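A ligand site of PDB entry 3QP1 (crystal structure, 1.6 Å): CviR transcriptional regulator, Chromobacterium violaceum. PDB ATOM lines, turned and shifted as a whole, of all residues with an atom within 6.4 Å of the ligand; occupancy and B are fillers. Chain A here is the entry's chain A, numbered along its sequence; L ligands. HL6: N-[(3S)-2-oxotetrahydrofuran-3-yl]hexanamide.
A nitrogen (N) of the ligand sits at hydrogen-bond distance from the side-chain carboxylate (OD2) of Asp 92, 2.8 Å away. The side-chain hydroxyl (OH) of Tyr 75 is in hydrogen-bond range of an oxygen (O3) of the ligand. The side-chain hydroxyl of Ser 150 is in hydrogen-bond range of an oxygen (O3) of the ligand (2.9 Å). The indole nitrogen of Trp 79 sits at hydrogen-bond distance from an oxygen (O1) of the ligand (3.0 Å).
The side-chain carboxylate (OD1) of Asp 92 sits at hydrogen-bond distance from the backbone NH (N) of Ile 94, 2.8 Å away. The side-chain hydroxyl (OH) of Tyr 83 sits at hydrogen-bond distance from the side-chain carboxylate (OD2) of Asp 92, at 2.6 Å. The backbone NH (N) of Ser 150 is in hydrogen-bond range of the backbone carbonyl oxygen (O) of Leu 52 (2.9 Å). OG of Ser 150 is in hydrogen-bond range of OG1 of Thr 135, 2.8 Å away. The backbone NH (N) of Met 130 is in hydrogen-bond range of the backbone carbonyl oxygen (O) of Ala 125. The indole nitrogen (NE1) of Trp 106 sits at hydrogen-bond distance from the side-chain hydroxyl (OG1) of Thr 135 (2.8 Å). The backbone NH (N) of Ile 148 sits at hydrogen-bond distance from the backbone carbonyl oxygen (O) of Ala 54, 2.9 Å away.
Leu 80 touches the ligand. Tyr 83 touches the ligand. CG1 of Ile 94 touches C3 of the ligand (3.5 Å). Leu 95 touches the ligand (CD2 to C6, 3.8 Å). Trp 106 touches the ligand. Phe 110 touches the ligand. Phe 121 touches the ligand. Ala 125 touches the ligand (CB to C2, 3.9 Å). O of Met 130 touches C2 of the ligand, at 3.4 Å. Ile 148 touches the ligand (CD1 to C7, 3.8 Å). 14 residues have an atom within 4 Å of the ligand: Tyr 75, Trp 79, Leu 80, Tyr 83, Asp 92, Ile 94, Leu 95, Trp 106, Phe 110, Phe 121, Ala 125, Met 130, Ile 148 and Ser 150. Along chain A the residues within 4 Å of the ligand span positions 75 to 150. The nearest printed residue that does not touch the ligand is Leu 52 (4.05 Å).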
ATOM      1  N   LEU A  52     -30.148  33.224   5.087  1.00  0.00           N
ATOM      2  CA  LEU A  52     -30.937  32.547   4.057  1.00  0.00           C
ATOM      3  C   LEU A  52     -31.939  31.619   4.731  1.00  0.00           C
ATOM      4  O   LEU A  52     -31.627  31.001   5.744  1.00  0.00           O
ATOM      5  CB  LEU A  52     -30.012  31.777   3.104  1.00  0.00           C
ATOM      6  CG  LEU A  52     -30.631  30.947   1.968  1.00  0.00           C
ATOM      7  CD1 LEU A  52     -29.770  31.008   0.688  1.00  0.00           C
ATOM      8  CD2 LEU A  52     -30.902  29.498   2.404  1.00  0.00           C
ATOM      9  N   ALA A  54     -34.623  28.372   3.808  1.00  0.00           N
ATOM     10  CA  ALA A  54     -35.049  27.412   2.791  1.00  0.00           C
ATOM     11  C   ALA A  54     -36.125  26.490   3.311  1.00  0.00           C
ATOM     12  O   ALA A  54     -36.136  26.153   4.491  1.00  0.00           O
ATOM     13  CB  ALA A  54     -33.877  26.588   2.228  1.00  0.00           C
ATOM     14  N   LEU A  67     -35.562  20.714  -2.442  1.00  0.00           N
ATOM     15  CA  LEU A  67     -35.769  22.116  -2.054  1.00  0.00           C
ATOM     16  C   LEU A  67     -37.016  22.672  -2.728  1.00  0.00           C
ATOM     17  O   LEU A  67     -37.181  22.563  -3.952  1.00  0.00           O
ATOM     18  CB  LEU A  67     -34.521  22.960  -2.385  1.00  0.00           C
ATOM     19  CG  LEU A  67     -33.289  22.686  -1.529  1.00  0.00           C
ATOM     20  CD1 LEU A  67     -32.014  23.187  -2.213  1.00  0.00           C
ATOM     21  CD2 LEU A  67     -33.436  23.315  -0.144  1.00  0.00           C
ATOM     22  N   VAL A  70     -36.184  28.671  -1.845  1.00  0.00           N
ATOM     23  CA  VAL A  70     -34.976  29.245  -1.247  1.00  0.00           C
ATOM     24  C   VAL A  70     -35.184  30.735  -1.198  1.00  0.00           C
ATOM     25  O   VAL A  70     -35.320  31.367  -2.254  1.00  0.00           O
ATOM     26  CB  VAL A  70     -33.715  28.910  -2.038  1.00  0.00           C
ATOM     27  CG1 VAL A  70     -32.489  29.552  -1.388  1.00  0.00           C
ATOM     28  CG2 VAL A  70     -33.535  27.401  -2.163  1.00  0.00           C
ATOM     29  N   TYR A  75     -27.252  36.334   1.548  1.00  0.00           N
ATOM     30  CA  TYR A  75     -26.091  35.624   0.997  1.00  0.00           C
ATOM     31  C   TYR A  75     -25.633  36.382  -0.243  1.00  0.00           C
ATOM     32  O   TYR A  75     -26.467  36.881  -1.008  1.00  0.00           O
ATOM     33  CB  TYR A  75     -26.462  34.201   0.601  1.00  0.00           C
ATOM     34  CG  TYR A  75     -26.390  33.166   1.696  1.00  0.00           C
ATOM     35  CD1 TYR A  75     -26.178  31.817   1.400  1.00  0.00           C
ATOM     36  CD2 TYR A  75     -26.571  33.528   3.040  1.00  0.00           C
ATOM     37  CE1 TYR A  75     -26.132  30.847   2.395  1.00  0.00           C
ATOM     38  CE2 TYR A  75     -26.515  32.556   4.056  1.00  0.00           C
ATOM     39  CZ  TYR A  75     -26.306  31.235   3.721  1.00  0.00           C
ATOM     40  OH  TYR A  75     -26.226  30.277   4.704  1.00  0.00           O
ATOM     41  N   TRP A  79     -22.101  33.892  -4.555  1.00  0.00           N
ATOM     42  CA  TRP A  79     -21.964  32.612  -3.862  1.00  0.00           C
ATOM     43  C   TRP A  79     -23.135  31.675  -4.180  1.00  0.00           C
ATOM     44  O   TRP A  79     -22.937  30.500  -4.470  1.00  0.00           O
ATOM     45  CB  TRP A  79     -21.805  32.818  -2.341  1.00  0.00           C
ATOM     46  CG  TRP A  79     -21.869  31.508  -1.560  1.00  0.00           C
ATOM     47  CD1 TRP A  79     -22.840  31.142  -0.638  1.00  0.00           C
ATOM     48  CD2 TRP A  79     -20.975  30.384  -1.651  1.00  0.00           C
ATOM     49  NE1 TRP A  79     -22.582  29.876  -0.164  1.00  0.00           N
ATOM     50  CE2 TRP A  79     -21.425  29.403  -0.737  1.00  0.00           C
ATOM     51  CE3 TRP A  79     -19.807  30.124  -2.404  1.00  0.00           C
ATOM     52  CZ2 TRP A  79     -20.776  28.173  -0.572  1.00  0.00           C
ATOM     53  CZ3 TRP A  79     -19.158  28.892  -2.226  1.00  0.00           C
ATOM     54  CH2 TRP A  79     -19.630  27.949  -1.323  1.00  0.00           C
ATOM     55  N   LEU A  80     -24.361  32.203  -4.120  1.00  0.00           N
ATOM     56  CA  LEU A  80     -25.539  31.404  -4.464  1.00  0.00           C
ATOM     57  C   LEU A  80     -25.508  30.904  -5.907  1.00  0.00           C
ATOM     58  O   LEU A  80     -25.811  29.740  -6.160  1.00  0.00           O
ATOM     59  CB  LEU A  80     -26.816  32.185  -4.213  1.00  0.00           C
ATOM     60  CG  LEU A  80     -27.405  32.142  -2.811  1.00  0.00           C
ATOM     61  CD1 LEU A  80     -28.890  32.479  -2.928  1.00  0.00           C
ATOM     62  CD2 LEU A  80     -27.255  30.767  -2.158  1.00  0.00           C
ATOM     63  N   TYR A  83     -23.145  28.140  -6.030  1.00  0.00           N
ATOM     64  CA  TYR A  83     -23.684  27.005  -5.284  1.00  0.00           C
ATOM     65  C   TYR A  83     -24.625  26.197  -6.176  1.00  0.00           C
ATOM     66  O   TYR A  83     -24.588  24.957  -6.200  1.00  0.00           O
ATOM     67  CB  TYR A  83     -24.424  27.550  -4.051  1.00  0.00           C
ATOM     68  CG  TYR A  83     -24.839  26.514  -3.034  1.00  0.00           C
ATOM     69  CD1 TYR A  83     -24.168  26.377  -1.824  1.00  0.00           C
ATOM     70  CD2 TYR A  83     -25.934  25.687  -3.276  1.00  0.00           C
ATOM     71  CE1 TYR A  83     -24.553  25.430  -0.872  1.00  0.00           C
ATOM     72  CE2 TYR A  83     -26.318  24.741  -2.338  1.00  0.00           C
ATOM     73  CZ  TYR A  83     -25.653  24.629  -1.140  1.00  0.00           C
ATOM     74  OH  TYR A  83     -26.055  23.677  -0.240  1.00  0.00           O
ATOM     75  N   MET A  84     -25.443  26.909  -6.935  1.00  0.00           N
ATOM     76  CA  MET A  84     -26.412  26.276  -7.816  1.00  0.00           C
ATOM     77  C   MET A  84     -25.711  25.665  -9.016  1.00  0.00           C
ATOM     78  O   MET A  84     -25.877  24.481  -9.312  1.00  0.00           O
ATOM     79  CB  MET A  84     -27.474  27.283  -8.265  1.00  0.00           C
ATOM     80  CG  MET A  84     -28.313  27.851  -7.123  1.00  0.00           C
ATOM     81  SD  MET A  84     -29.179  26.572  -6.210  1.00  0.00           S
ATOM     82  CE  MET A  84     -30.397  26.050  -7.424  1.00  0.00           C
ATOM     83  N   ASP A  92     -22.877  19.798   0.305  1.00  0.00           N
ATOM     84  CA  ASP A  92     -22.944  20.695   1.471  1.00  0.00           C
ATOM     85  C   ASP A  92     -23.443  19.918   2.691  1.00  0.00           C
ATOM     86  O   ASP A  92     -24.595  19.510   2.709  1.00  0.00           O
ATOM     87  CB  ASP A  92     -23.886  21.850   1.141  1.00  0.00           C
ATOM     88  CG  ASP A  92     -24.040  22.847   2.291  1.00  0.00           C
ATOM     89  OD1 ASP A  92     -23.464  22.641   3.386  1.00  0.00           O
ATOM     90  OD2 ASP A  92     -24.712  23.858   2.027  1.00  0.00           O
ATOM     91  N   PRO A  93     -22.581  19.736   3.710  1.00  0.00           N
ATOM     92  CA  PRO A  93     -22.954  19.006   4.931  1.00  0.00           C
ATOM     93  C   PRO A  93     -24.208  19.595   5.596  1.00  0.00           C
ATOM     94  O   PRO A  93     -24.950  18.865   6.255  1.00  0.00           O
ATOM     95  CB  PRO A  93     -21.723  19.181   5.826  1.00  0.00           C
ATOM     96  CG  PRO A  93     -20.611  19.388   4.853  1.00  0.00           C
ATOM     97  CD  PRO A  93     -21.192  20.231   3.790  1.00  0.00           C
ATOM     98  N   ILE A  94     -24.449  20.890   5.398  1.00  0.00           N
ATOM     99  CA  ILE A  94     -25.597  21.566   6.024  1.00  0.00           C
ATOM    100  C   ILE A  94     -26.920  21.006   5.498  1.00  0.00           C
ATOM    101  O   ILE A  94     -27.911  20.895   6.255  1.00  0.00           O
ATOM    102  CB  ILE A  94     -25.542  23.121   5.856  1.00  0.00           C
ATOM    103  CG1 ILE A  94     -24.246  23.708   6.455  1.00  0.00           C
ATOM    104  CG2 ILE A  94     -26.825  23.805   6.431  1.00  0.00           C
ATOM    105  CD1 ILE A  94     -23.744  23.067   7.714  1.00  0.00           C
ATOM    106  N   LEU A  95     -26.950  20.635   4.223  1.00  0.00           N
ATOM    107  CA  LEU A  95     -28.184  20.076   3.653  1.00  0.00           C
ATOM    108  C   LEU A  95     -28.408  18.622   4.056  1.00  0.00           C
ATOM    109  O   LEU A  95     -29.437  18.027   3.697  1.00  0.00           O
ATOM    110  CB  LEU A  95     -28.238  20.260   2.129  1.00  0.00           C
ATOM    111  CG  LEU A  95     -28.365  21.692   1.620  1.00  0.00           C
ATOM    112  CD1 LEU A  95     -28.764  21.697   0.192  1.00  0.00           C
ATOM    113  CD2 LEU A  95     -29.386  22.491   2.427  1.00  0.00           C
ATOM    114  N   TRP A 106     -21.567  25.337  12.012  1.00  0.00           N
ATOM    115  CA  TRP A 106     -20.942  24.856  10.786  1.00  0.00           C
ATOM    116  C   TRP A 106     -19.502  24.364  11.002  1.00  0.00           C
ATOM    117  O   TRP A 106     -19.149  23.295  10.500  1.00  0.00           O
ATOM    118  CB  TRP A 106     -20.939  25.921   9.699  1.00  0.00           C
ATOM    119  CG  TRP A 106     -22.277  26.436   9.257  1.00  0.00           C
ATOM    120  CD1 TRP A 106     -23.534  25.982   9.641  1.00  0.00           C
ATOM    121  CD2 TRP A 106     -22.493  27.479   8.302  1.00  0.00           C
ATOM    122  NE1 TRP A 106     -24.497  26.718   8.988  1.00  0.00           N
ATOM    123  CE2 TRP A 106     -23.896  27.644   8.171  1.00  0.00           C
ATOM    124  CE3 TRP A 106     -21.628  28.316   7.572  1.00  0.00           C
ATOM    125  CZ2 TRP A 106     -24.455  28.605   7.317  1.00  0.00           C
ATOM    126  CZ3 TRP A 106     -22.180  29.271   6.718  1.00  0.00           C
ATOM    127  CH2 TRP A 106     -23.595  29.404   6.611  1.00  0.00           C
ATOM    128  N   PHE A 110     -18.281  20.897   9.884  1.00  0.00           N
ATOM    129  CA  PHE A 110     -17.288  20.843   8.807  1.00  0.00           C
ATOM    130  C   PHE A 110     -16.042  20.054   9.203  1.00  0.00           C
ATOM    131  O   PHE A 110     -15.509  19.268   8.412  1.00  0.00           O
ATOM    132  CB  PHE A 110     -16.892  22.257   8.369  1.00  0.00           C
ATOM    133  CG  PHE A 110     -17.971  22.995   7.608  1.00  0.00           C
ATOM    134  CD1 PHE A 110     -19.117  22.334   7.168  1.00  0.00           C
ATOM    135  CD2 PHE A 110     -17.817  24.341   7.301  1.00  0.00           C
ATOM    136  CE1 PHE A 110     -20.087  23.015   6.451  1.00  0.00           C
ATOM    137  CE2 PHE A 110     -18.783  25.026   6.592  1.00  0.00           C
ATOM    138  CZ  PHE A 110     -19.921  24.359   6.152  1.00  0.00           C
ATOM    139  N   PHE A 121     -15.972  21.289  -1.147  1.00  0.00           N
ATOM    140  CA  PHE A 121     -16.997  22.274  -0.861  1.00  0.00           C
ATOM    141  C   PHE A 121     -16.641  23.155   0.348  1.00  0.00           C
ATOM    142  O   PHE A 121     -16.782  24.379   0.305  1.00  0.00           O
ATOM    143  CB  PHE A 121     -18.346  21.594  -0.589  1.00  0.00           C
ATOM    144  CG  PHE A 121     -19.352  22.531  -0.008  1.00  0.00           C
ATOM    145  CD1 PHE A 121     -20.032  23.435  -0.820  1.00  0.00           C
ATOM    146  CD2 PHE A 121     -19.571  22.569   1.380  1.00  0.00           C
ATOM    147  CE1 PHE A 121     -20.944  24.346  -0.270  1.00  0.00           C
ATOM    148  CE2 PHE A 121     -20.487  23.492   1.939  1.00  0.00           C
ATOM    149  CZ  PHE A 121     -21.167  24.363   1.108  1.00  0.00           C
ATOM    150  N   ALA A 125     -16.359  27.069   0.378  1.00  0.00           N
ATOM    151  CA  ALA A 125     -17.210  27.871   1.226  1.00  0.00           C
ATOM    152  C   ALA A 125     -16.361  28.805   2.077  1.00  0.00           C
ATOM    153  O   ALA A 125     -16.631  30.007   2.173  1.00  0.00           O
ATOM    154  CB  ALA A 125     -18.104  26.976   2.105  1.00  0.00           C
ATOM    155  N   MET A 130     -17.868  31.757   4.099  1.00  0.00           N
ATOM    156  CA  MET A 130     -18.955  30.873   4.550  1.00  0.00           C
ATOM    157  C   MET A 130     -18.423  29.670   5.344  1.00  0.00           C
ATOM    158  O   MET A 130     -19.068  28.629   5.410  1.00  0.00           O
ATOM    159  CB  MET A 130     -19.746  30.360   3.325  1.00  0.00           C
ATOM    160  CG  MET A 130     -20.364  31.456   2.483  1.00  0.00           C
ATOM    161  SD  MET A 130     -21.350  32.500   3.558  1.00  0.00           S
ATOM    162  CE  MET A 130     -22.157  33.559   2.441  1.00  0.00           C
ATOM    163  N   GLY A 131     -17.257  29.803   5.944  1.00  0.00           N
ATOM    164  CA  GLY A 131     -16.659  28.701   6.698  1.00  0.00           C
ATOM    165  C   GLY A 131     -17.238  28.560   8.089  1.00  0.00           C
ATOM    166  O   GLY A 131     -17.081  27.515   8.747  1.00  0.00           O
ATOM    167  N   THR A 135     -26.989  26.883  11.541  1.00  0.00           N
ATOM    168  CA  THR A 135     -28.267  26.593  10.886  1.00  0.00           C
ATOM    169  C   THR A 135     -29.270  26.072  11.901  1.00  0.00           C
ATOM    170  O   THR A 135     -29.015  25.086  12.566  1.00  0.00           O
ATOM    171  CB  THR A 135     -28.088  25.580   9.721  1.00  0.00           C
ATOM    172  OG1 THR A 135     -27.239  26.180   8.748  1.00  0.00           O
ATOM    173  CG2 THR A 135     -29.437  25.249   9.049  1.00  0.00           C
ATOM    174  N   ILE A 148     -34.995  25.396   7.038  1.00  0.00           N
ATOM    175  CA  ILE A 148     -33.715  25.737   7.650  1.00  0.00           C
ATOM    176  C   ILE A 148     -33.555  27.259   7.614  1.00  0.00           C
ATOM    177  O   ILE A 148     -33.940  27.929   6.646  1.00  0.00           O
ATOM    178  CB  ILE A 148     -32.515  25.081   6.937  1.00  0.00           C
ATOM    179  CG1 ILE A 148     -32.509  25.325   5.424  1.00  0.00           C
ATOM    180  CG2 ILE A 148     -32.456  23.584   7.291  1.00  0.00           C
ATOM    181  CD1 ILE A 148     -31.145  24.924   4.747  1.00  0.00           C
ATOM    182  N   SER A 150     -30.348  29.734   7.969  1.00  0.00           N
ATOM    183  CA  SER A 150     -28.896  29.760   8.042  1.00  0.00           C
ATOM    184  C   SER A 150     -28.401  31.168   8.224  1.00  0.00           C
ATOM    185  O   SER A 150     -28.868  32.080   7.542  1.00  0.00           O
ATOM    186  CB  SER A 150     -28.298  29.182   6.759  1.00  0.00           C
ATOM    187  OG  SER A 150     -28.371  27.770   6.764  1.00  0.00           O
ATOM    188  N   ILE A 151     -27.440  31.341   9.113  1.00  0.00           N
ATOM    189  CA  ILE A 151     -26.798  32.629   9.306  1.00  0.00           C
ATOM    190  C   ILE A 151     -25.286  32.411   9.303  1.00  0.00           C
ATOM    191  O   ILE A 151     -24.767  31.611  10.095  1.00  0.00           O
ATOM    192  CB  ILE A 151     -27.284  33.316  10.609  1.00  0.00           C
ATOM    193  CG1 ILE A 151     -28.807  33.489  10.556  1.00  0.00           C
ATOM    194  CG2 ILE A 151     -26.570  34.662  10.772  1.00  0.00           C
ATOM    195  CD1 ILE A 151     -29.357  34.210  11.745  1.00  0.00           C
HETATM  196  N   HL6 L   1     -25.144  26.103   3.563  1.00  0.00           N
HETATM  197  C1  HL6 L   1     -23.441  27.632   2.726  1.00  0.00           C
HETATM  198  O1  HL6 L   1     -24.059  28.165   1.824  1.00  0.00           O
HETATM  199  C2  HL6 L   1     -21.564  26.891   3.930  1.00  0.00           C
HETATM  200  O2  HL6 L   1     -22.019  27.605   2.769  1.00  0.00           O
HETATM  201  C3  HL6 L   1     -22.797  26.095   4.389  1.00  0.00           C
HETATM  202  O3  HL6 L   1     -26.647  27.548   4.427  1.00  0.00           O
HETATM  203  C4  HL6 L   1     -23.996  26.914   3.914  1.00  0.00           C
HETATM  204  C5  HL6 L   1     -26.385  26.493   3.849  1.00  0.00           C
HETATM  205  C6  HL6 L   1     -27.469  25.574   3.404  1.00  0.00           C
HETATM  206  C7  HL6 L   1     -28.454  26.273   2.495  1.00  0.00           C
HETATM  207  C8  HL6 L   1     -27.847  26.513   1.133  1.00  0.00           C
HETATM  208  C9  HL6 L   1     -28.966  26.500   0.101  1.00  0.00           C
HETATM  209  C10 HL6 L   1     -28.619  27.421  -1.042  1.00  0.00           C
